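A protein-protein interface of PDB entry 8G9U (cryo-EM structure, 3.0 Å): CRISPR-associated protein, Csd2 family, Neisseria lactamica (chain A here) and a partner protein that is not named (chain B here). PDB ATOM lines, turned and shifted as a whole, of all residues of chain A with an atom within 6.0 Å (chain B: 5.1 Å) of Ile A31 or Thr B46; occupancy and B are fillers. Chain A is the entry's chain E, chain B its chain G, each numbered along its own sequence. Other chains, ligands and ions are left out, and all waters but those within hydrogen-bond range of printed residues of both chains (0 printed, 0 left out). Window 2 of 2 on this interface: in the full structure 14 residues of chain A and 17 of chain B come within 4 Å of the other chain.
ND2 of Asn B90 sits close to OE1 of Gln A34, 3.4 Å away.
The backbone NH of Asp A22 lies within hydrogen-bond range of the backbone carbonyl oxygen of Leu A28 (2.4 Å). The backbone NH (N) of Gln A34 is in hydrogen-bond range of the side-chain carboxylate (OD1) of Asp A32 (3.3 Å). The backbone carbonyl oxygen of Ser B45 lies within hydrogen-bond range of a ring nitrogen (ND1) of His B91 (3.3 Å). N of Ile B48 lies close to O of Pro B89 (3.5 Å).
CD1 of Leu A28 touches O of Ala B49, 3.4 Å away. CG2 of Thr B46 touches CD1 of Ile A31 (3.9 Å). Ala B49 touches Ile A31 (CB to CD1, 3.6 Å). Pro A33 touches Thr B46 (CG to OG1, 3.0 Å). Ile B48 touches Pro A33 (CD1 to O, 3.2 Å). CB of Pro A33 touches O of Asn B90 (3.0 Å). CG of Pro A33 touches CD2 of His B91 (3.4 Å). CG of Gln A34 touches CB of His B91, at 3.4 Å.
Printed residues of chain B within 4 Å of Leu A28: Ala B49. Ile A31 touches just these residues of chain B: Thr B46 (3.9 Å) and Ala B49 (3.6 Å). Printed residues of chain B within 4 Å of Pro A33: Thr B46 (3.0 Å), Ile B48 (3.2 Å), Asn B90 (3.0 Å) and His B91 (3.4 Å). Thr B46 touches just these residues of chain A: Ile A31 and Pro A33. Of the printed residues of chain A, Ile B48 touches Pro A33. Pro B89 touches none of the printed residues of chain A. Printed residues of chain A within 4 Å of Asn B90: Pro A33 (3.0 Å) and Gln A34 (3.2 Å). Of the printed residues of chain A, His B91 touches Pro A33 (3.4 Å) and Gln A34 (3.4 Å). Gln B97 touches none of the printed residues of chain A. The nearest residue of chain B that does not touch Ile A31 is Ile B48 (4.1 Å).
Printed residues of chain B that touch a printed residue of chain A: Thr B46, Ile B48, Ala B49, Asn B90 and His B91. Hydrophobic or aromatic side chains of chain B within 4 Å of the printed part of chain A: Ile B48, Ala B49 and His B91. Of the 14 printed residues of chain A, 4 touch a printed residue of chain B. Hydrophobic or aromatic side chains of chain A within 4 Å of the printed part of chain B: Leu A28, Ile A31 and Pro A33.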
ATOM      1  N   ASP A  22     -20.001  35.755  23.333  1.00  0.00           N
ATOM      2  CA  ASP A  22     -20.917  36.320  24.304  1.00  0.00           C
ATOM      3  C   ASP A  22     -20.087  36.920  25.421  1.00  0.00           C
ATOM      4  O   ASP A  22     -19.417  36.174  26.143  1.00  0.00           O
ATOM      5  CB  ASP A  22     -21.850  35.253  24.847  1.00  0.00           C
ATOM      6  CG  ASP A  22     -23.116  35.829  25.441  1.00  0.00           C
ATOM      7  OD1 ASP A  22     -23.229  37.066  25.519  1.00  0.00           O
ATOM      8  OD2 ASP A  22     -24.003  35.044  25.830  1.00  0.00           O
ATOM      9  N   LEU A  28     -17.396  33.002  24.584  1.00  0.00           N
ATOM     10  CA  LEU A  28     -18.089  31.856  24.024  1.00  0.00           C
ATOM     11  C   LEU A  28     -19.063  32.320  22.954  1.00  0.00           C
ATOM     12  O   LEU A  28     -19.732  33.343  23.131  1.00  0.00           O
ATOM     13  CB  LEU A  28     -18.848  31.096  25.109  1.00  0.00           C
ATOM     14  CG  LEU A  28     -18.103  29.963  25.799  1.00  0.00           C
ATOM     15  CD1 LEU A  28     -18.761  29.642  27.112  1.00  0.00           C
ATOM     16  CD2 LEU A  28     -18.094  28.748  24.906  1.00  0.00           C
ATOM     17  N   PRO A  29     -19.164  31.609  21.839  1.00  0.00           N
ATOM     18  CA  PRO A  29     -20.127  32.002  20.815  1.00  0.00           C
ATOM     19  C   PRO A  29     -21.505  32.113  21.433  1.00  0.00           C
ATOM     20  O   PRO A  29     -21.905  31.279  22.245  1.00  0.00           O
ATOM     21  CB  PRO A  29     -20.047  30.864  19.798  1.00  0.00           C
ATOM     22  CG  PRO A  29     -18.735  30.239  20.035  1.00  0.00           C
ATOM     23  CD  PRO A  29     -18.475  30.362  21.491  1.00  0.00           C
ATOM     24  N   ARG A  30     -22.209  33.186  21.098  1.00  0.00           N
ATOM     25  CA  ARG A  30     -23.540  33.349  21.646  1.00  0.00           C
ATOM     26  C   ARG A  30     -24.374  32.158  21.240  1.00  0.00           C
ATOM     27  O   ARG A  30     -24.669  31.980  20.059  1.00  0.00           O
ATOM     28  CB  ARG A  30     -24.198  34.623  21.154  1.00  0.00           C
ATOM     29  CG  ARG A  30     -23.456  35.849  21.485  1.00  0.00           C
ATOM     30  CD  ARG A  30     -24.324  37.014  21.215  1.00  0.00           C
ATOM     31  NE  ARG A  30     -23.599  38.254  21.368  1.00  0.00           N
ATOM     32  CZ  ARG A  30     -23.667  39.000  22.453  1.00  0.00           C
ATOM     33  NH1 ARG A  30     -24.423  38.617  23.463  1.00  0.00           N
ATOM     34  NH2 ARG A  30     -22.986  40.124  22.524  1.00  0.00           N
ATOM     35  N   ILE A  31     -24.728  31.340  22.183  1.00  0.00           N
ATOM     36  CA  ILE A  31     -25.600  30.218  21.910  1.00  0.00           C
ATOM     37  C   ILE A  31     -26.985  30.594  22.383  1.00  0.00           C
ATOM     38  O   ILE A  31     -27.151  31.343  23.349  1.00  0.00           O
ATOM     39  CB  ILE A  31     -25.115  28.930  22.600  1.00  0.00           C
ATOM     40  CG1 ILE A  31     -25.119  29.118  24.112  1.00  0.00           C
ATOM     41  CG2 ILE A  31     -23.733  28.556  22.118  1.00  0.00           C
ATOM     42  CD1 ILE A  31     -24.886  27.850  24.865  1.00  0.00           C
ATOM     43  N   ASP A  32     -27.984  30.111  21.684  1.00  0.00           N
ATOM     44  CA  ASP A  32     -29.300  30.115  22.269  1.00  0.00           C
ATOM     45  C   ASP A  32     -29.293  29.022  23.317  1.00  0.00           C
ATOM     46  O   ASP A  32     -29.054  27.857  22.981  1.00  0.00           O
ATOM     47  CB  ASP A  32     -30.377  29.864  21.236  1.00  0.00           C
ATOM     48  CG  ASP A  32     -31.758  30.163  21.758  1.00  0.00           C
ATOM     49  OD1 ASP A  32     -32.038  29.885  22.937  1.00  0.00           O
ATOM     50  OD2 ASP A  32     -32.576  30.685  20.985  1.00  0.00           O
ATOM     51  N   PRO A  33     -29.518  29.338  24.559  1.00  0.00           N
ATOM     52  CA  PRO A  33     -29.463  28.320  25.605  1.00  0.00           C
ATOM     53  C   PRO A  33     -30.355  27.143  25.289  1.00  0.00           C
ATOM     54  O   PRO A  33     -29.899  26.008  25.140  1.00  0.00           O
ATOM     55  CB  PRO A  33     -29.972  29.065  26.837  1.00  0.00           C
ATOM     56  CG  PRO A  33     -29.845  30.480  26.523  1.00  0.00           C
ATOM     57  CD  PRO A  33     -29.954  30.642  25.067  1.00  0.00           C
ATOM     58  N   GLN A  34     -31.635  27.431  25.129  1.00  0.00           N
ATOM     59  CA  GLN A  34     -32.631  26.379  25.120  1.00  0.00           C
ATOM     60  C   GLN A  34     -32.658  25.590  23.832  1.00  0.00           C
ATOM     61  O   GLN A  34     -33.509  24.708  23.697  1.00  0.00           O
ATOM     62  CB  GLN A  34     -33.996  26.982  25.394  1.00  0.00           C
ATOM     63  CG  GLN A  34     -34.227  27.308  26.853  1.00  0.00           C
ATOM     64  CD  GLN A  34     -34.560  26.090  27.696  1.00  0.00           C
ATOM     65  OE1 GLN A  34     -34.322  24.953  27.293  1.00  0.00           O
ATOM     66  NE2 GLN A  34     -35.096  26.328  28.886  1.00  0.00           N
ATOM     67  N   GLY A  36     -29.228  25.403  21.964  1.00  0.00           N
ATOM     68  CA  GLY A  36     -27.850  25.284  21.548  1.00  0.00           C
ATOM     69  C   GLY A  36     -27.509  25.980  20.253  1.00  0.00           C
ATOM     70  O   GLY A  36     -26.336  25.992  19.868  1.00  0.00           O
ATOM     71  N   GLU A  37     -28.491  26.553  19.566  1.00  0.00           N
ATOM     72  CA  GLU A  37     -28.226  27.273  18.333  1.00  0.00           C
ATOM     73  C   GLU A  37     -27.406  28.514  18.628  1.00  0.00           C
ATOM     74  O   GLU A  37     -27.682  29.247  19.578  1.00  0.00           O
ATOM     75  CB  GLU A  37     -29.533  27.669  17.651  1.00  0.00           C
ATOM     76  CG  GLU A  37     -30.159  26.578  16.808  1.00  0.00           C
ATOM     77  CD  GLU A  37     -31.445  27.027  16.144  1.00  0.00           C
ATOM     78  OE1 GLU A  37     -31.795  28.217  16.267  1.00  0.00           O
ATOM     79  OE2 GLU A  37     -32.105  26.191  15.490  1.00  0.00           O
ATOM     80  N   GLY A  38     -26.390  28.747  17.810  1.00  0.00           N
ATOM     81  CA  GLY A  38     -25.573  29.924  17.989  1.00  0.00           C
ATOM     82  C   GLY A  38     -26.318  31.187  17.611  1.00  0.00           C
ATOM     83  O   GLY A  38     -27.239  31.179  16.798  1.00  0.00           O
ATOM     84  N   LEU A  39     -25.912  32.293  18.218  1.00  0.00           N
ATOM     85  CA  LEU A  39     -26.411  33.605  17.844  1.00  0.00           C
ATOM     86  C   LEU A  39     -25.258  34.490  17.428  1.00  0.00           C
ATOM     87  O   LEU A  39     -24.170  34.425  18.001  1.00  0.00           O
ATOM     88  CB  LEU A  39     -27.186  34.283  18.961  1.00  0.00           C
ATOM     89  CG  LEU A  39     -28.624  33.815  19.113  1.00  0.00           C
ATOM     90  CD1 LEU A  39     -28.691  32.414  19.595  1.00  0.00           C
ATOM     91  CD2 LEU A  39     -29.359  34.699  20.055  1.00  0.00           C
ATOM     92  N   ILE A 139     -24.552  24.729  17.630  1.00  0.00           N
ATOM     93  CA  ILE A 139     -23.114  24.842  17.442  1.00  0.00           C
ATOM     94  C   ILE A 139     -22.422  24.213  18.637  1.00  0.00           C
ATOM     95  O   ILE A 139     -22.743  24.523  19.790  1.00  0.00           O
ATOM     96  CB  ILE A 139     -22.693  26.308  17.261  1.00  0.00           C
ATOM     97  CG1 ILE A 139     -23.258  27.167  18.386  1.00  0.00           C
ATOM     98  CG2 ILE A 139     -23.180  26.825  15.932  1.00  0.00           C
ATOM     99  CD1 ILE A 139     -22.477  28.408  18.628  1.00  0.00           C
ATOM    100  N   THR A 141     -19.577  24.599  20.298  1.00  0.00           N
ATOM    101  CA  THR A 141     -18.445  25.464  20.596  1.00  0.00           C
ATOM    102  C   THR A 141     -17.326  24.657  21.231  1.00  0.00           C
ATOM    103  O   THR A 141     -17.516  24.069  22.299  1.00  0.00           O
ATOM    104  CB  THR A 141     -18.860  26.582  21.539  1.00  0.00           C
ATOM    105  OG1 THR A 141     -19.018  26.046  22.854  1.00  0.00           O
ATOM    106  CG2 THR A 141     -20.180  27.149  21.106  1.00  0.00           C
ATOM    107  N   SER B  42     -23.729  34.892  31.712  1.00  0.00           N
ATOM    108  CA  SER B  42     -24.456  33.765  31.152  1.00  0.00           C
ATOM    109  C   SER B  42     -24.610  32.634  32.146  1.00  0.00           C
ATOM    110  O   SER B  42     -25.609  31.916  32.105  1.00  0.00           O
ATOM    111  CB  SER B  42     -23.751  33.245  29.914  1.00  0.00           C
ATOM    112  OG  SER B  42     -22.441  32.886  30.270  1.00  0.00           O
ATOM    113  N   ALA B  43     -23.647  32.459  33.048  1.00  0.00           N
ATOM    114  CA  ALA B  43     -23.823  31.477  34.105  1.00  0.00           C
ATOM    115  C   ALA B  43     -25.123  31.711  34.838  1.00  0.00           C
ATOM    116  O   ALA B  43     -25.806  30.757  35.216  1.00  0.00           O
ATOM    117  CB  ALA B  43     -22.654  31.536  35.078  1.00  0.00           C
ATOM    118  N   SER B  44     -25.500  32.968  35.009  1.00  0.00           N
ATOM    119  CA  SER B  44     -26.781  33.305  35.587  1.00  0.00           C
ATOM    120  C   SER B  44     -27.930  33.074  34.630  1.00  0.00           C
ATOM    121  O   SER B  44     -29.056  32.873  35.082  1.00  0.00           O
ATOM    122  CB  SER B  44     -26.778  34.762  36.031  1.00  0.00           C
ATOM    123  OG  SER B  44     -28.031  35.131  36.567  1.00  0.00           O
ATOM    124  N   SER B  45     -27.686  33.083  33.336  1.00  0.00           N
ATOM    125  CA  SER B  45     -28.779  32.956  32.388  1.00  0.00           C
ATOM    126  C   SER B  45     -28.688  31.724  31.512  1.00  0.00           C
ATOM    127  O   SER B  45     -29.704  31.086  31.252  1.00  0.00           O
ATOM    128  CB  SER B  45     -28.858  34.204  31.506  1.00  0.00           C
ATOM    129  OG  SER B  45     -27.697  34.360  30.718  1.00  0.00           O
ATOM    130  N   THR B  46     -27.499  31.358  31.064  1.00  0.00           N
ATOM    131  CA  THR B  46     -27.302  30.230  30.161  1.00  0.00           C
ATOM    132  C   THR B  46     -26.281  29.294  30.783  1.00  0.00           C
ATOM    133  O   THR B  46     -25.129  29.225  30.345  1.00  0.00           O
ATOM    134  CB  THR B  46     -26.840  30.718  28.792  1.00  0.00           C
ATOM    135  OG1 THR B  46     -27.771  31.685  28.299  1.00  0.00           O
ATOM    136  CG2 THR B  46     -26.743  29.569  27.823  1.00  0.00           C
ATOM    137  N   PRO B  47     -26.668  28.569  31.828  1.00  0.00           N
ATOM    138  CA  PRO B  47     -25.686  27.754  32.544  1.00  0.00           C
ATOM    139  C   PRO B  47     -25.014  26.717  31.686  1.00  0.00           C
ATOM    140  O   PRO B  47     -23.865  26.366  31.960  1.00  0.00           O
ATOM    141  CB  PRO B  47     -26.525  27.112  33.645  1.00  0.00           C
ATOM    142  CG  PRO B  47     -27.591  28.060  33.856  1.00  0.00           C
ATOM    143  CD  PRO B  47     -27.964  28.553  32.509  1.00  0.00           C
ATOM    144  N   ILE B  48     -25.682  26.203  30.657  1.00  0.00           N
ATOM    145  CA  ILE B  48     -25.017  25.247  29.786  1.00  0.00           C
ATOM    146  C   ILE B  48     -23.863  25.898  29.051  1.00  0.00           C
ATOM    147  O   ILE B  48     -22.853  25.244  28.773  1.00  0.00           O
ATOM    148  CB  ILE B  48     -26.006  24.621  28.799  1.00  0.00           C
ATOM    149  CG1 ILE B  48     -26.629  25.709  27.942  1.00  0.00           C
ATOM    150  CG2 ILE B  48     -27.035  23.818  29.524  1.00  0.00           C
ATOM    151  CD1 ILE B  48     -27.298  25.179  26.746  1.00  0.00           C
ATOM    152  N   ALA B  49     -23.992  27.179  28.703  1.00  0.00           N
ATOM    153  CA  ALA B  49     -22.934  27.845  27.958  1.00  0.00           C
ATOM    154  C   ALA B  49     -21.616  27.755  28.702  1.00  0.00           C
ATOM    155  O   ALA B  49     -20.675  27.094  28.256  1.00  0.00           O
ATOM    156  CB  ALA B  49     -23.299  29.304  27.708  1.00  0.00           C
ATOM    157  N   VAL B  50     -21.545  28.380  29.870  1.00  0.00           N
ATOM    158  CA  VAL B  50     -20.315  28.425  30.629  1.00  0.00           C
ATOM    159  C   VAL B  50     -20.097  27.158  31.439  1.00  0.00           C
ATOM    160  O   VAL B  50     -19.068  26.510  31.281  1.00  0.00           O
ATOM    161  CB  VAL B  50     -20.284  29.675  31.523  1.00  0.00           C
ATOM    162  CG1 VAL B  50     -20.150  30.888  30.669  1.00  0.00           C
ATOM    163  CG2 VAL B  50     -21.555  29.765  32.267  1.00  0.00           C
ATOM    164  N   PRO B  89     -29.216  23.591  33.509  1.00  0.00           N
ATOM    165  CA  PRO B  89     -30.354  23.919  32.662  1.00  0.00           C
ATOM    166  C   PRO B  89     -29.923  24.728  31.464  1.00  0.00           C
ATOM    167  O   PRO B  89     -29.001  25.540  31.533  1.00  0.00           O
ATOM    168  CB  PRO B  89     -31.260  24.729  33.590  1.00  0.00           C
ATOM    169  CG  PRO B  89     -30.349  25.280  34.582  1.00  0.00           C
ATOM    170  CD  PRO B  89     -29.313  24.242  34.812  1.00  0.00           C
ATOM    171  N   ASN B  90     -30.605  24.483  30.351  1.00  0.00           N
ATOM    172  CA  ASN B  90     -30.287  25.182  29.119  1.00  0.00           C
ATOM    173  C   ASN B  90     -30.333  26.683  29.348  1.00  0.00           C
ATOM    174  O   ASN B  90     -29.309  27.368  29.275  1.00  0.00           O
ATOM    175  CB  ASN B  90     -31.265  24.751  28.031  1.00  0.00           C
ATOM    176  CG  ASN B  90     -30.802  23.523  27.284  1.00  0.00           C
ATOM    177  OD1 ASN B  90     -29.622  23.191  27.278  1.00  0.00           O
ATOM    178  ND2 ASN B  90     -31.742  22.823  26.666  1.00  0.00           N
ATOM    179  N   HIS B  91     -31.504  27.202  29.685  1.00  0.00           N
ATOM    180  CA  HIS B  91     -31.674  28.588  30.085  1.00  0.00           C
ATOM    181  C   HIS B  91     -32.273  28.621  31.477  1.00  0.00           C
ATOM    182  O   HIS B  91     -33.297  27.980  31.722  1.00  0.00           O
ATOM    183  CB  HIS B  91     -32.587  29.328  29.117  1.00  0.00           C
ATOM    184  CG  HIS B  91     -32.578  30.807  29.287  1.00  0.00           C
ATOM    185  ND1 HIS B  91     -32.895  31.422  30.483  1.00  0.00           N
ATOM    186  CD2 HIS B  91     -32.329  31.808  28.415  1.00  0.00           C
ATOM    187  CE1 HIS B  91     -32.816  32.728  30.342  1.00  0.00           C
ATOM    188  NE2 HIS B  91     -32.475  32.991  29.090  1.00  0.00           N
ATOM    189  N   LEU B  92     -31.654  29.369  32.380  1.00  0.00           N
ATOM    190  CA  LEU B  92     -32.191  29.476  33.727  1.00  0.00           C
ATOM    191  C   LEU B  92     -33.540  30.169  33.692  1.00  0.00           C
ATOM    192  O   LEU B  92     -33.689  31.231  33.085  1.00  0.00           O
ATOM    193  CB  LEU B  92     -31.231  30.228  34.637  1.00  0.00           C
ATOM    194  CG  LEU B  92     -30.293  29.337  35.439  1.00  0.00           C
ATOM    195  CD1 LEU B  92     -29.482  30.118  36.434  1.00  0.00           C
ATOM    196  CD2 LEU B  92     -31.091  28.296  36.146  1.00  0.00           C
ATOM    197  N   GLN B  97     -33.361  32.582  37.350  1.00  0.00           N
ATOM    198  CA  GLN B  97     -32.469  33.673  36.984  1.00  0.00           C
ATOM    199  C   GLN B  97     -32.030  34.416  38.226  1.00  0.00           C
ATOM    200  O   GLN B  97     -30.833  34.571  38.485  1.00  0.00           O
ATOM    201  CB  GLN B  97     -33.181  34.671  36.069  1.00  0.00           C
ATOM    202  CG  GLN B  97     -32.988  34.570  34.580  1.00  0.00           C
ATOM    203  CD  GLN B  97     -31.667  34.032  34.182  1.00  0.00           C
ATOM    204  OE1 GLN B  97     -31.596  33.092  33.407  1.00  0.00           O
ATOM    205  NE2 GLN B  97     -30.607  34.564  34.761  1.00  0.00           N
